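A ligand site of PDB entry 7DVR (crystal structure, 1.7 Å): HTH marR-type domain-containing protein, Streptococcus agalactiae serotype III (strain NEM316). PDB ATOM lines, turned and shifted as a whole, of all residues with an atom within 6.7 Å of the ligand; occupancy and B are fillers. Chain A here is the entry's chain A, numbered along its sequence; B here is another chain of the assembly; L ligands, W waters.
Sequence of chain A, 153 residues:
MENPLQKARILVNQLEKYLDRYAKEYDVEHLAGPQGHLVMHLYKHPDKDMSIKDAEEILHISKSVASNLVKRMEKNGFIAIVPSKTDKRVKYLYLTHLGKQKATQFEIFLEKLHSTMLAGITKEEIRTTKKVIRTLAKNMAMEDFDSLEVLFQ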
ATOM      1  N   LEU A  15       4.086 -13.101 -11.601  1.00  0.00           N
ATOM      2  CA  LEU A  15       5.375 -13.373 -12.194  1.00  0.00           C
ATOM      3  C   LEU A  15       5.493 -12.754 -13.580  1.00  0.00           C
ATOM      4  O   LEU A  15       6.560 -12.231 -13.840  1.00  0.00           O
ATOM      5  CB  LEU A  15       5.521 -14.877 -12.224  1.00  0.00           C
ATOM      6  CG  LEU A  15       6.714 -15.341 -13.011  1.00  0.00           C
ATOM      7  CD1 LEU A  15       7.989 -14.842 -12.386  1.00  0.00           C
ATOM      8  CD2 LEU A  15       6.676 -16.877 -13.106  1.00  0.00           C
ATOM      9  N   LEU A  19       8.461 -10.055 -14.518  1.00  0.00           N
ATOM     10  CA  LEU A  19       9.428 -10.274 -15.583  1.00  0.00           C
ATOM     11  C   LEU A  19       9.371  -9.184 -16.612  1.00  0.00           C
ATOM     12  O   LEU A  19      10.395  -8.752 -17.061  1.00  0.00           O
ATOM     13  CB  LEU A  19       8.970 -11.613 -16.162  1.00  0.00           C
ATOM     14  CG  LEU A  19       9.772 -12.263 -17.261  1.00  0.00           C
ATOM     15  CD1 LEU A  19      11.273 -12.210 -16.979  1.00  0.00           C
ATOM     16  CD2 LEU A  19       9.251 -13.697 -17.346  1.00  0.00           C
ATOM     17  N   LEU A  31      13.048  -9.915 -25.437  1.00  0.00           N
ATOM     18  CA  LEU A  31      14.043 -10.982 -25.496  1.00  0.00           C
ATOM     19  C   LEU A  31      13.702 -12.112 -24.539  1.00  0.00           C
ATOM     20  O   LEU A  31      14.401 -13.154 -24.596  1.00  0.00           O
ATOM     21  CB  LEU A  31      15.422 -10.436 -25.237  1.00  0.00           C
ATOM     22  CG  LEU A  31      15.992  -9.693 -26.423  1.00  0.00           C
ATOM     23  CD1 LEU A  31      16.942  -8.629 -25.936  1.00  0.00           C
ATOM     24  CD2 LEU A  31      16.695 -10.622 -27.409  1.00  0.00           C
ATOM     25  N   ALA A  32      12.653 -11.964 -23.749  1.00  0.00           N
ATOM     26  CA  ALA A  32      12.284 -12.995 -22.760  1.00  0.00           C
ATOM     27  C   ALA A  32      12.007 -14.326 -23.423  1.00  0.00           C
ATOM     28  O   ALA A  32      12.335 -15.298 -22.790  1.00  0.00           O
ATOM     29  CB  ALA A  32      11.084 -12.578 -21.954  1.00  0.00           C
ATOM     30  N   GLY A  33      11.455 -14.391 -24.645  1.00  0.00           N
ATOM     31  CA  GLY A  33      11.100 -15.701 -25.222  1.00  0.00           C
ATOM     32  C   GLY A  33      12.025 -16.212 -26.325  1.00  0.00           C
ATOM     33  O   GLY A  33      13.201 -16.518 -26.125  1.00  0.00           O
ATOM     34  N   PHE A 106      21.282  -9.130 -22.081  1.00  0.00           N
ATOM     35  CA  PHE A 106      20.305 -10.194 -21.739  1.00  0.00           C
ATOM     36  C   PHE A 106      20.953 -11.166 -20.777  1.00  0.00           C
ATOM     37  O   PHE A 106      20.286 -11.660 -19.864  1.00  0.00           O
ATOM     38  CB  PHE A 106      19.835 -10.961 -22.981  1.00  0.00           C
ATOM     39  CG  PHE A 106      18.642 -11.856 -22.721  1.00  0.00           C
ATOM     40  CD1 PHE A 106      17.430 -11.342 -22.293  1.00  0.00           C
ATOM     41  CD2 PHE A 106      18.723 -13.224 -22.979  1.00  0.00           C
ATOM     42  CE1 PHE A 106      16.327 -12.172 -22.087  1.00  0.00           C
ATOM     43  CE2 PHE A 106      17.626 -14.050 -22.762  1.00  0.00           C
ATOM     44  CZ  PHE A 106      16.423 -13.525 -22.333  1.00  0.00           C
ATOM     45  N   PHE A 109      20.999  -9.591 -17.311  1.00  0.00           N
ATOM     46  CA  PHE A 109      19.599  -9.641 -16.835  1.00  0.00           C
ATOM     47  C   PHE A 109      19.254 -11.031 -16.293  1.00  0.00           C
ATOM     48  O   PHE A 109      18.709 -11.115 -15.214  1.00  0.00           O
ATOM     49  CB  PHE A 109      18.623  -9.262 -17.958  1.00  0.00           C
ATOM     50  CG  PHE A 109      17.171  -9.572 -17.686  1.00  0.00           C
ATOM     51  CD1 PHE A 109      16.409  -8.810 -16.805  1.00  0.00           C
ATOM     52  CD2 PHE A 109      16.523 -10.621 -18.333  1.00  0.00           C
ATOM     53  CE1 PHE A 109      15.075  -9.128 -16.586  1.00  0.00           C
ATOM     54  CE2 PHE A 109      15.175 -10.902 -18.153  1.00  0.00           C
ATOM     55  CZ  PHE A 109      14.451 -10.168 -17.249  1.00  0.00           C
ATOM     56  N   LEU A 110      19.558 -12.079 -17.039  1.00  0.00           N
ATOM     57  CA  LEU A 110      19.141 -13.432 -16.603  1.00  0.00           C
ATOM     58  C   LEU A 110      19.893 -13.770 -15.323  1.00  0.00           C
ATOM     59  O   LEU A 110      19.289 -14.433 -14.446  1.00  0.00           O
ATOM     60  CB  LEU A 110      19.401 -14.456 -17.703  1.00  0.00           C
ATOM     61  CG  LEU A 110      18.396 -14.433 -18.859  1.00  0.00           C
ATOM     62  CD1 LEU A 110      18.742 -15.476 -19.898  1.00  0.00           C
ATOM     63  CD2 LEU A 110      16.972 -14.658 -18.404  1.00  0.00           C
ATOM     64  N   LEU A 113      18.296 -11.642 -12.523  1.00  0.00           N
ATOM     65  CA  LEU A 113      16.923 -12.124 -12.304  1.00  0.00           C
ATOM     66  C   LEU A 113      16.919 -13.362 -11.410  1.00  0.00           C
ATOM     67  O   LEU A 113      16.187 -13.378 -10.462  1.00  0.00           O
ATOM     68  CB  LEU A 113      16.257 -12.420 -13.637  1.00  0.00           C
ATOM     69  CG  LEU A 113      14.910 -13.149 -13.610  1.00  0.00           C
ATOM     70  CD1 LEU A 113      13.810 -12.252 -13.085  1.00  0.00           C
ATOM     71  CD2 LEU A 113      14.524 -13.600 -15.003  1.00  0.00           C
ATOM     72  N   HIS A 114      17.643 -14.386 -11.797  1.00  0.00           N
ATOM     73  CA  HIS A 114      17.804 -15.639 -11.005  1.00  0.00           C
ATOM     74  C   HIS A 114      18.372 -15.341  -9.610  1.00  0.00           C
ATOM     75  O   HIS A 114      17.708 -15.776  -8.659  1.00  0.00           O
ATOM     76  CB  HIS A 114      18.591 -16.675 -11.792  1.00  0.00           C
ATOM     77  CG  HIS A 114      17.797 -17.246 -12.922  1.00  0.00           C
ATOM     78  ND1 HIS A 114      17.717 -16.613 -14.163  1.00  0.00           N
ATOM     79  CD2 HIS A 114      17.038 -18.373 -13.005  1.00  0.00           C
ATOM     80  CE1 HIS A 114      16.972 -17.363 -14.959  1.00  0.00           C
ATOM     81  NE2 HIS A 114      16.539 -18.398 -14.277  1.00  0.00           N
ATOM     82  N   MET A 117      15.400 -13.849  -7.755  1.00  0.00           N
ATOM     83  CA  MET A 117      14.260 -14.774  -7.564  1.00  0.00           C
ATOM     84  C   MET A 117      14.611 -15.922  -6.616  1.00  0.00           C
ATOM     85  O   MET A 117      13.699 -16.490  -5.923  1.00  0.00           O
ATOM     86  CB  MET A 117      13.924 -15.385  -8.914  1.00  0.00           C
ATOM     87  CG  MET A 117      13.113 -14.478  -9.799  1.00  0.00           C
ATOM     88  SD  MET A 117      12.480 -15.431 -11.200  1.00  0.00           S
ATOM     89  CE  MET A 117      13.987 -15.872 -12.031  1.00  0.00           C
ATOM     90  N   LEU A 118      15.871 -16.324  -6.664  1.00  0.00           N
ATOM     91  CA  LEU A 118      16.237 -17.597  -6.027  1.00  0.00           C
ATOM     92  C   LEU A 118      16.933 -17.313  -4.714  1.00  0.00           C
ATOM     93  O   LEU A 118      17.428 -18.267  -4.085  1.00  0.00           O
ATOM     94  CB  LEU A 118      17.134 -18.457  -6.932  1.00  0.00           C
ATOM     95  CG  LEU A 118      16.523 -18.944  -8.249  1.00  0.00           C
ATOM     96  CD1 LEU A 118      17.514 -19.822  -9.039  1.00  0.00           C
ATOM     97  CD2 LEU A 118      15.238 -19.693  -7.988  1.00  0.00           C
ATOM     98  N   LYS A 123      19.756 -25.509  -3.469  1.00  0.00           N
ATOM     99  CA  LYS A 123      19.736 -26.414  -4.640  1.00  0.00           C
ATOM    100  C   LYS A 123      18.871 -27.622  -4.287  1.00  0.00           C
ATOM    101  O   LYS A 123      18.232 -28.159  -5.203  1.00  0.00           O
ATOM    102  CB  LYS A 123      21.132 -26.862  -5.057  1.00  0.00           C
ATOM    103  CG  LYS A 123      22.174 -25.750  -5.122  1.00  0.00           C
ATOM    104  CD  LYS A 123      22.942 -25.645  -6.422  1.00  0.00           C
ATOM    105  CE  LYS A 123      22.206 -24.829  -7.469  1.00  0.00           C
ATOM    106  NZ  LYS A 123      22.775 -25.017  -8.831  1.00  0.00           N
ATOM    107  N   ILE A 126      15.107 -26.745  -4.488  1.00  0.00           N
ATOM    108  CA  ILE A 126      14.734 -26.678  -5.952  1.00  0.00           C
ATOM    109  C   ILE A 126      14.469 -28.115  -6.410  1.00  0.00           C
ATOM    110  O   ILE A 126      13.409 -28.378  -6.995  1.00  0.00           O
ATOM    111  CB  ILE A 126      15.834 -26.046  -6.819  1.00  0.00           C
ATOM    112  CG1 ILE A 126      16.059 -24.561  -6.490  1.00  0.00           C
ATOM    113  CG2 ILE A 126      15.564 -26.239  -8.311  1.00  0.00           C
ATOM    114  CD1 ILE A 126      14.824 -23.757  -6.389  1.00  0.00           C
ATOM    115  N   LYS A 130      10.961 -29.418  -7.716  1.00  0.00           N
ATOM    116  CA  LYS A 130      10.923 -30.046  -9.063  1.00  0.00           C
ATOM    117  C   LYS A 130      10.341 -31.454  -8.998  1.00  0.00           C
ATOM    118  O   LYS A 130       9.536 -31.824  -9.845  1.00  0.00           O
ATOM    119  CB  LYS A 130      12.302 -30.113  -9.690  1.00  0.00           C
ATOM    120  CG  LYS A 130      12.800 -28.774 -10.239  1.00  0.00           C
ATOM    121  CD  LYS A 130      14.015 -28.929 -11.125  1.00  0.00           C
ATOM    122  CE  LYS A 130      14.414 -27.641 -11.831  1.00  0.00           C
ATOM    123  NZ  LYS A 130      15.492 -27.889 -12.820  1.00  0.00           N
ATOM    124  N   MET B   1      13.871 -21.215 -15.652  1.00  0.00           N
ATOM    125  CA  MET B   1      13.967 -22.075 -16.793  1.00  0.00           C
ATOM    126  C   MET B   1      13.303 -21.389 -17.995  1.00  0.00           C
ATOM    127  O   MET B   1      12.292 -20.662 -17.864  1.00  0.00           O
ATOM    128  CB  MET B   1      13.285 -23.417 -16.486  1.00  0.00           C
ATOM    129  CG  MET B   1      13.647 -24.012 -15.083  1.00  0.00           C
ATOM    130  SD  MET B   1      12.261 -23.977 -13.880  1.00  0.00           S
ATOM    131  CE  MET B   1      13.161 -24.064 -12.352  1.00  0.00           C
ATOM    132  N   GLU B   2      13.797 -21.716 -19.169  1.00  0.00           N
ATOM    133  CA  GLU B   2      13.268 -21.147 -20.422  1.00  0.00           C
ATOM    134  C   GLU B   2      11.743 -21.306 -20.496  1.00  0.00           C
ATOM    135  O   GLU B   2      11.208 -22.318 -20.085  1.00  0.00           O
ATOM    136  CB  GLU B   2      13.964 -21.833 -21.586  1.00  0.00           C
ATOM    137  CG  GLU B   2      13.920 -21.042 -22.874  1.00  0.00           C
ATOM    138  CD  GLU B   2      15.207 -21.128 -23.688  1.00  0.00           C
ATOM    139  OE1 GLU B   2      15.629 -20.076 -24.226  1.00  0.00           O
ATOM    140  OE2 GLU B   2      15.805 -22.236 -23.743  1.00  0.00           O
ATOM    141  N   ASN B   3      11.068 -20.306 -21.050  1.00  0.00           N
ATOM    142  CA  ASN B   3       9.596 -20.310 -21.280  1.00  0.00           C
ATOM    143  C   ASN B   3       8.878 -20.680 -19.978  1.00  0.00           C
ATOM    144  O   ASN B   3       8.083 -21.623 -19.919  1.00  0.00           O
ATOM    145  CB  ASN B   3       9.215 -21.248 -22.446  1.00  0.00           C
ATOM    146  CG  ASN B   3       9.890 -20.881 -23.757  1.00  0.00           C
ATOM    147  OD1 ASN B   3       9.736 -19.775 -24.261  1.00  0.00           O
ATOM    148  ND2 ASN B   3      10.662 -21.801 -24.314  1.00  0.00           N
ATOM    149  N   PRO B   4       9.142 -19.911 -18.911  1.00  0.00           N
ATOM    150  CA  PRO B   4       8.575 -20.120 -17.576  1.00  0.00           C
ATOM    151  C   PRO B   4       7.044 -20.072 -17.490  1.00  0.00           C
ATOM    152  O   PRO B   4       6.421 -20.941 -16.886  1.00  0.00           O
ATOM    153  CB  PRO B   4       9.095 -18.924 -16.757  1.00  0.00           C
ATOM    154  CG  PRO B   4       9.912 -18.048 -17.687  1.00  0.00           C
ATOM    155  CD  PRO B   4      10.100 -18.799 -18.989  1.00  0.00           C
ATOM    156  N   LEU B 136       9.465 -17.504  -3.350  1.00  0.00           N
ATOM    157  CA  LEU B 136       9.414 -16.981  -4.738  1.00  0.00           C
ATOM    158  C   LEU B 136       8.431 -15.809  -4.772  1.00  0.00           C
ATOM    159  O   LEU B 136       8.804 -14.755  -5.309  1.00  0.00           O
ATOM    160  CB  LEU B 136       8.949 -18.103  -5.679  1.00  0.00           C
ATOM    161  CG  LEU B 136      10.021 -19.129  -6.054  1.00  0.00           C
ATOM    162  CD1 LEU B 136       9.490 -20.168  -7.029  1.00  0.00           C
ATOM    163  CD2 LEU B 136      11.242 -18.455  -6.640  1.00  0.00           C
ATOM    164  N   MET B 140       9.556 -11.770  -5.583  1.00  0.00           N
ATOM    165  CA  MET B 140       9.115 -11.126  -6.850  1.00  0.00           C
ATOM    166  C   MET B 140       7.888 -10.257  -6.607  1.00  0.00           C
ATOM    167  O   MET B 140       7.151  -9.984  -7.581  1.00  0.00           O
ATOM    168  CB  MET B 140       8.765 -12.192  -7.889  1.00  0.00           C
ATOM    169  CG  MET B 140       7.357 -12.753  -7.691  1.00  0.00           C
ATOM    170  SD  MET B 140       6.809 -13.963  -8.918  1.00  0.00           S
ATOM    171  CE  MET B 140       5.308 -14.554  -8.140  1.00  0.00           C
HETATM  172  C1  LIG L   1      17.854 -21.825 -14.804  1.00  0.00           C
HETATM  173  C2  LIG L   1      16.213 -19.247 -18.422  1.00  0.00           C
HETATM  174  C3  LIG L   1      12.934 -17.425 -15.469  1.00  0.00           C
HETATM  175  C4  LIG L   1      14.128 -20.596 -12.132  1.00  0.00           C
HETATM  176  C5  LIG L   1      17.694 -21.230 -15.998  1.00  0.00           C
HETATM  177  C6  LIG L   1      18.541 -21.448 -17.073  1.00  0.00           C
HETATM  178  C7  LIG L   1      18.071 -20.722 -18.092  1.00  0.00           C
HETATM  179  C8  LIG L   1      16.936 -20.080 -17.647  1.00  0.00           C
HETATM  180  C9  LIG L   1      18.683 -20.660 -19.460  1.00  0.00           C
HETATM  181  C10 LIG L   1      19.769 -22.327 -17.112  1.00  0.00           C
HETATM  182  C11 LIG L   1      21.026 -21.514 -16.758  1.00  0.00           C
HETATM  183  C12 LIG L   1      22.292 -22.359 -16.778  1.00  0.00           C
HETATM  184  O1  LIG L   1      22.505 -23.129 -17.752  1.00  0.00           O
HETATM  185  O2  LIG L   1      23.128 -22.301 -15.851  1.00  0.00           O
HETATM  186  C13 LIG L   1      15.184 -18.525 -17.869  1.00  0.00           C
HETATM  187  C14 LIG L   1      14.533 -17.542 -18.623  1.00  0.00           C
HETATM  188  C15 LIG L   1      13.616 -17.000 -17.794  1.00  0.00           C
HETATM  189  C16 LIG L   1      13.731 -17.702 -16.539  1.00  0.00           C
HETATM  190  C17 LIG L   1      14.837 -17.210 -20.056  1.00  0.00           C
HETATM  191  C18 LIG L   1      12.624 -15.978 -18.057  1.00  0.00           C
HETATM  192  C19 LIG L   1      12.421 -15.528 -19.280  1.00  0.00           C
HETATM  193  C20 LIG L   1      12.933 -18.165 -14.333  1.00  0.00           C
HETATM  194  C21 LIG L   1      11.988 -18.076 -13.345  1.00  0.00           C
HETATM  195  C22 LIG L   1      12.320 -19.000 -12.396  1.00  0.00           C
HETATM  196  C23 LIG L   1      13.491 -19.624 -12.815  1.00  0.00           C
HETATM  197  C24 LIG L   1      10.821 -17.146 -13.374  1.00  0.00           C
HETATM  198  C25 LIG L   1      11.674 -19.255 -11.112  1.00  0.00           C
HETATM  199  C26 LIG L   1      10.807 -18.389 -10.594  1.00  0.00           C
HETATM  200  C27 LIG L   1      15.262 -21.167 -12.633  1.00  0.00           C
HETATM  201  C28 LIG L   1      16.008 -22.105 -11.845  1.00  0.00           C
HETATM  202  C29 LIG L   1      17.067 -22.444 -12.576  1.00  0.00           C
HETATM  203  C30 LIG L   1      16.934 -21.694 -13.811  1.00  0.00           C
HETATM  204  C31 LIG L   1      15.710 -22.609 -10.458  1.00  0.00           C
HETATM  205  C32 LIG L   1      18.145 -23.415 -12.175  1.00  0.00           C
HETATM  206  C33 LIG L   1      19.511 -22.710 -12.054  1.00  0.00           C
HETATM  207  C34 LIG L   1      20.602 -23.734 -11.777  1.00  0.00           C
HETATM  208  O3  LIG L   1      20.716 -24.189 -10.613  1.00  0.00           O
HETATM  209  O4  LIG L   1      21.386 -24.108 -12.674  1.00  0.00           O
HETATM  210  N1  LIG L   1      16.713 -20.392 -16.365  1.00  0.00           N
HETATM  211  N2  LIG L   1      14.675 -18.573 -16.661  1.00  0.00           N
HETATM  212  N3  LIG L   1      13.830 -19.081 -13.986  1.00  0.00           N
HETATM  213  N4  LIG L   1      15.855 -20.952 -13.774  1.00  0.00           N
HETATM  214 FE1  LIG L   1      15.296 -19.825 -15.121  1.00  0.00          FE
HETATM  215  O   HOH W   1      12.052 -17.656 -22.067  1.00  0.00           O
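A ring nitrogen (NE2) of His 114 is bound to an iron atom (FE1) of the ligand, 2.1 Å away.
O3 of the ligand is in salt-bridge range of NZ of Lys 123 (2.8 Å).
FE1 of the ligand is bound by N of Met 1 of chain B, 2.1 Å away.
The backbone carbonyl oxygen (O) of Leu 110 sits at hydrogen-bond distance from a ring nitrogen (ND1) of His 114 (2.7 Å).
Leu 15 touches the ligand (CD1 to C24, 3.8 Å).
Ala 32 touches the ligand.
CD2 of Leu 110 touches C17 of the ligand (3.7 Å).
Met 117 touches the ligand (SD to C24, 3.2 Å).
Leu 118 touches the ligand (CD1 to C31, 3.6 Å).
Glu 2 of chain B touches the ligand (N to C2, 3.5 Å).
Pro 4 of chain B touches the ligand.
Leu 136 of chain B touches the ligand (CD2 to C26, 3.98 Å).
Hydrophobic or aromatic side chains within 4 Å of the ligand: Leu 15, Leu 110, His 114, Met 117, Leu 118, Met 1 of chain B, Pro 4 of chain B and Leu 136 of chain B.
Within 4 Å of the ligand: Leu 15, Ala 32, Leu 110, His 114, Met 117, Leu 118, Lys 123, Met 1 of chain B, Glu 2 of chain B, Pro 4 of chain B and Leu 136 of chain B.
Water W1 bridges O of Ala 32 (2.5 Å) and N of Asn 3 of chain B (3.0 Å).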
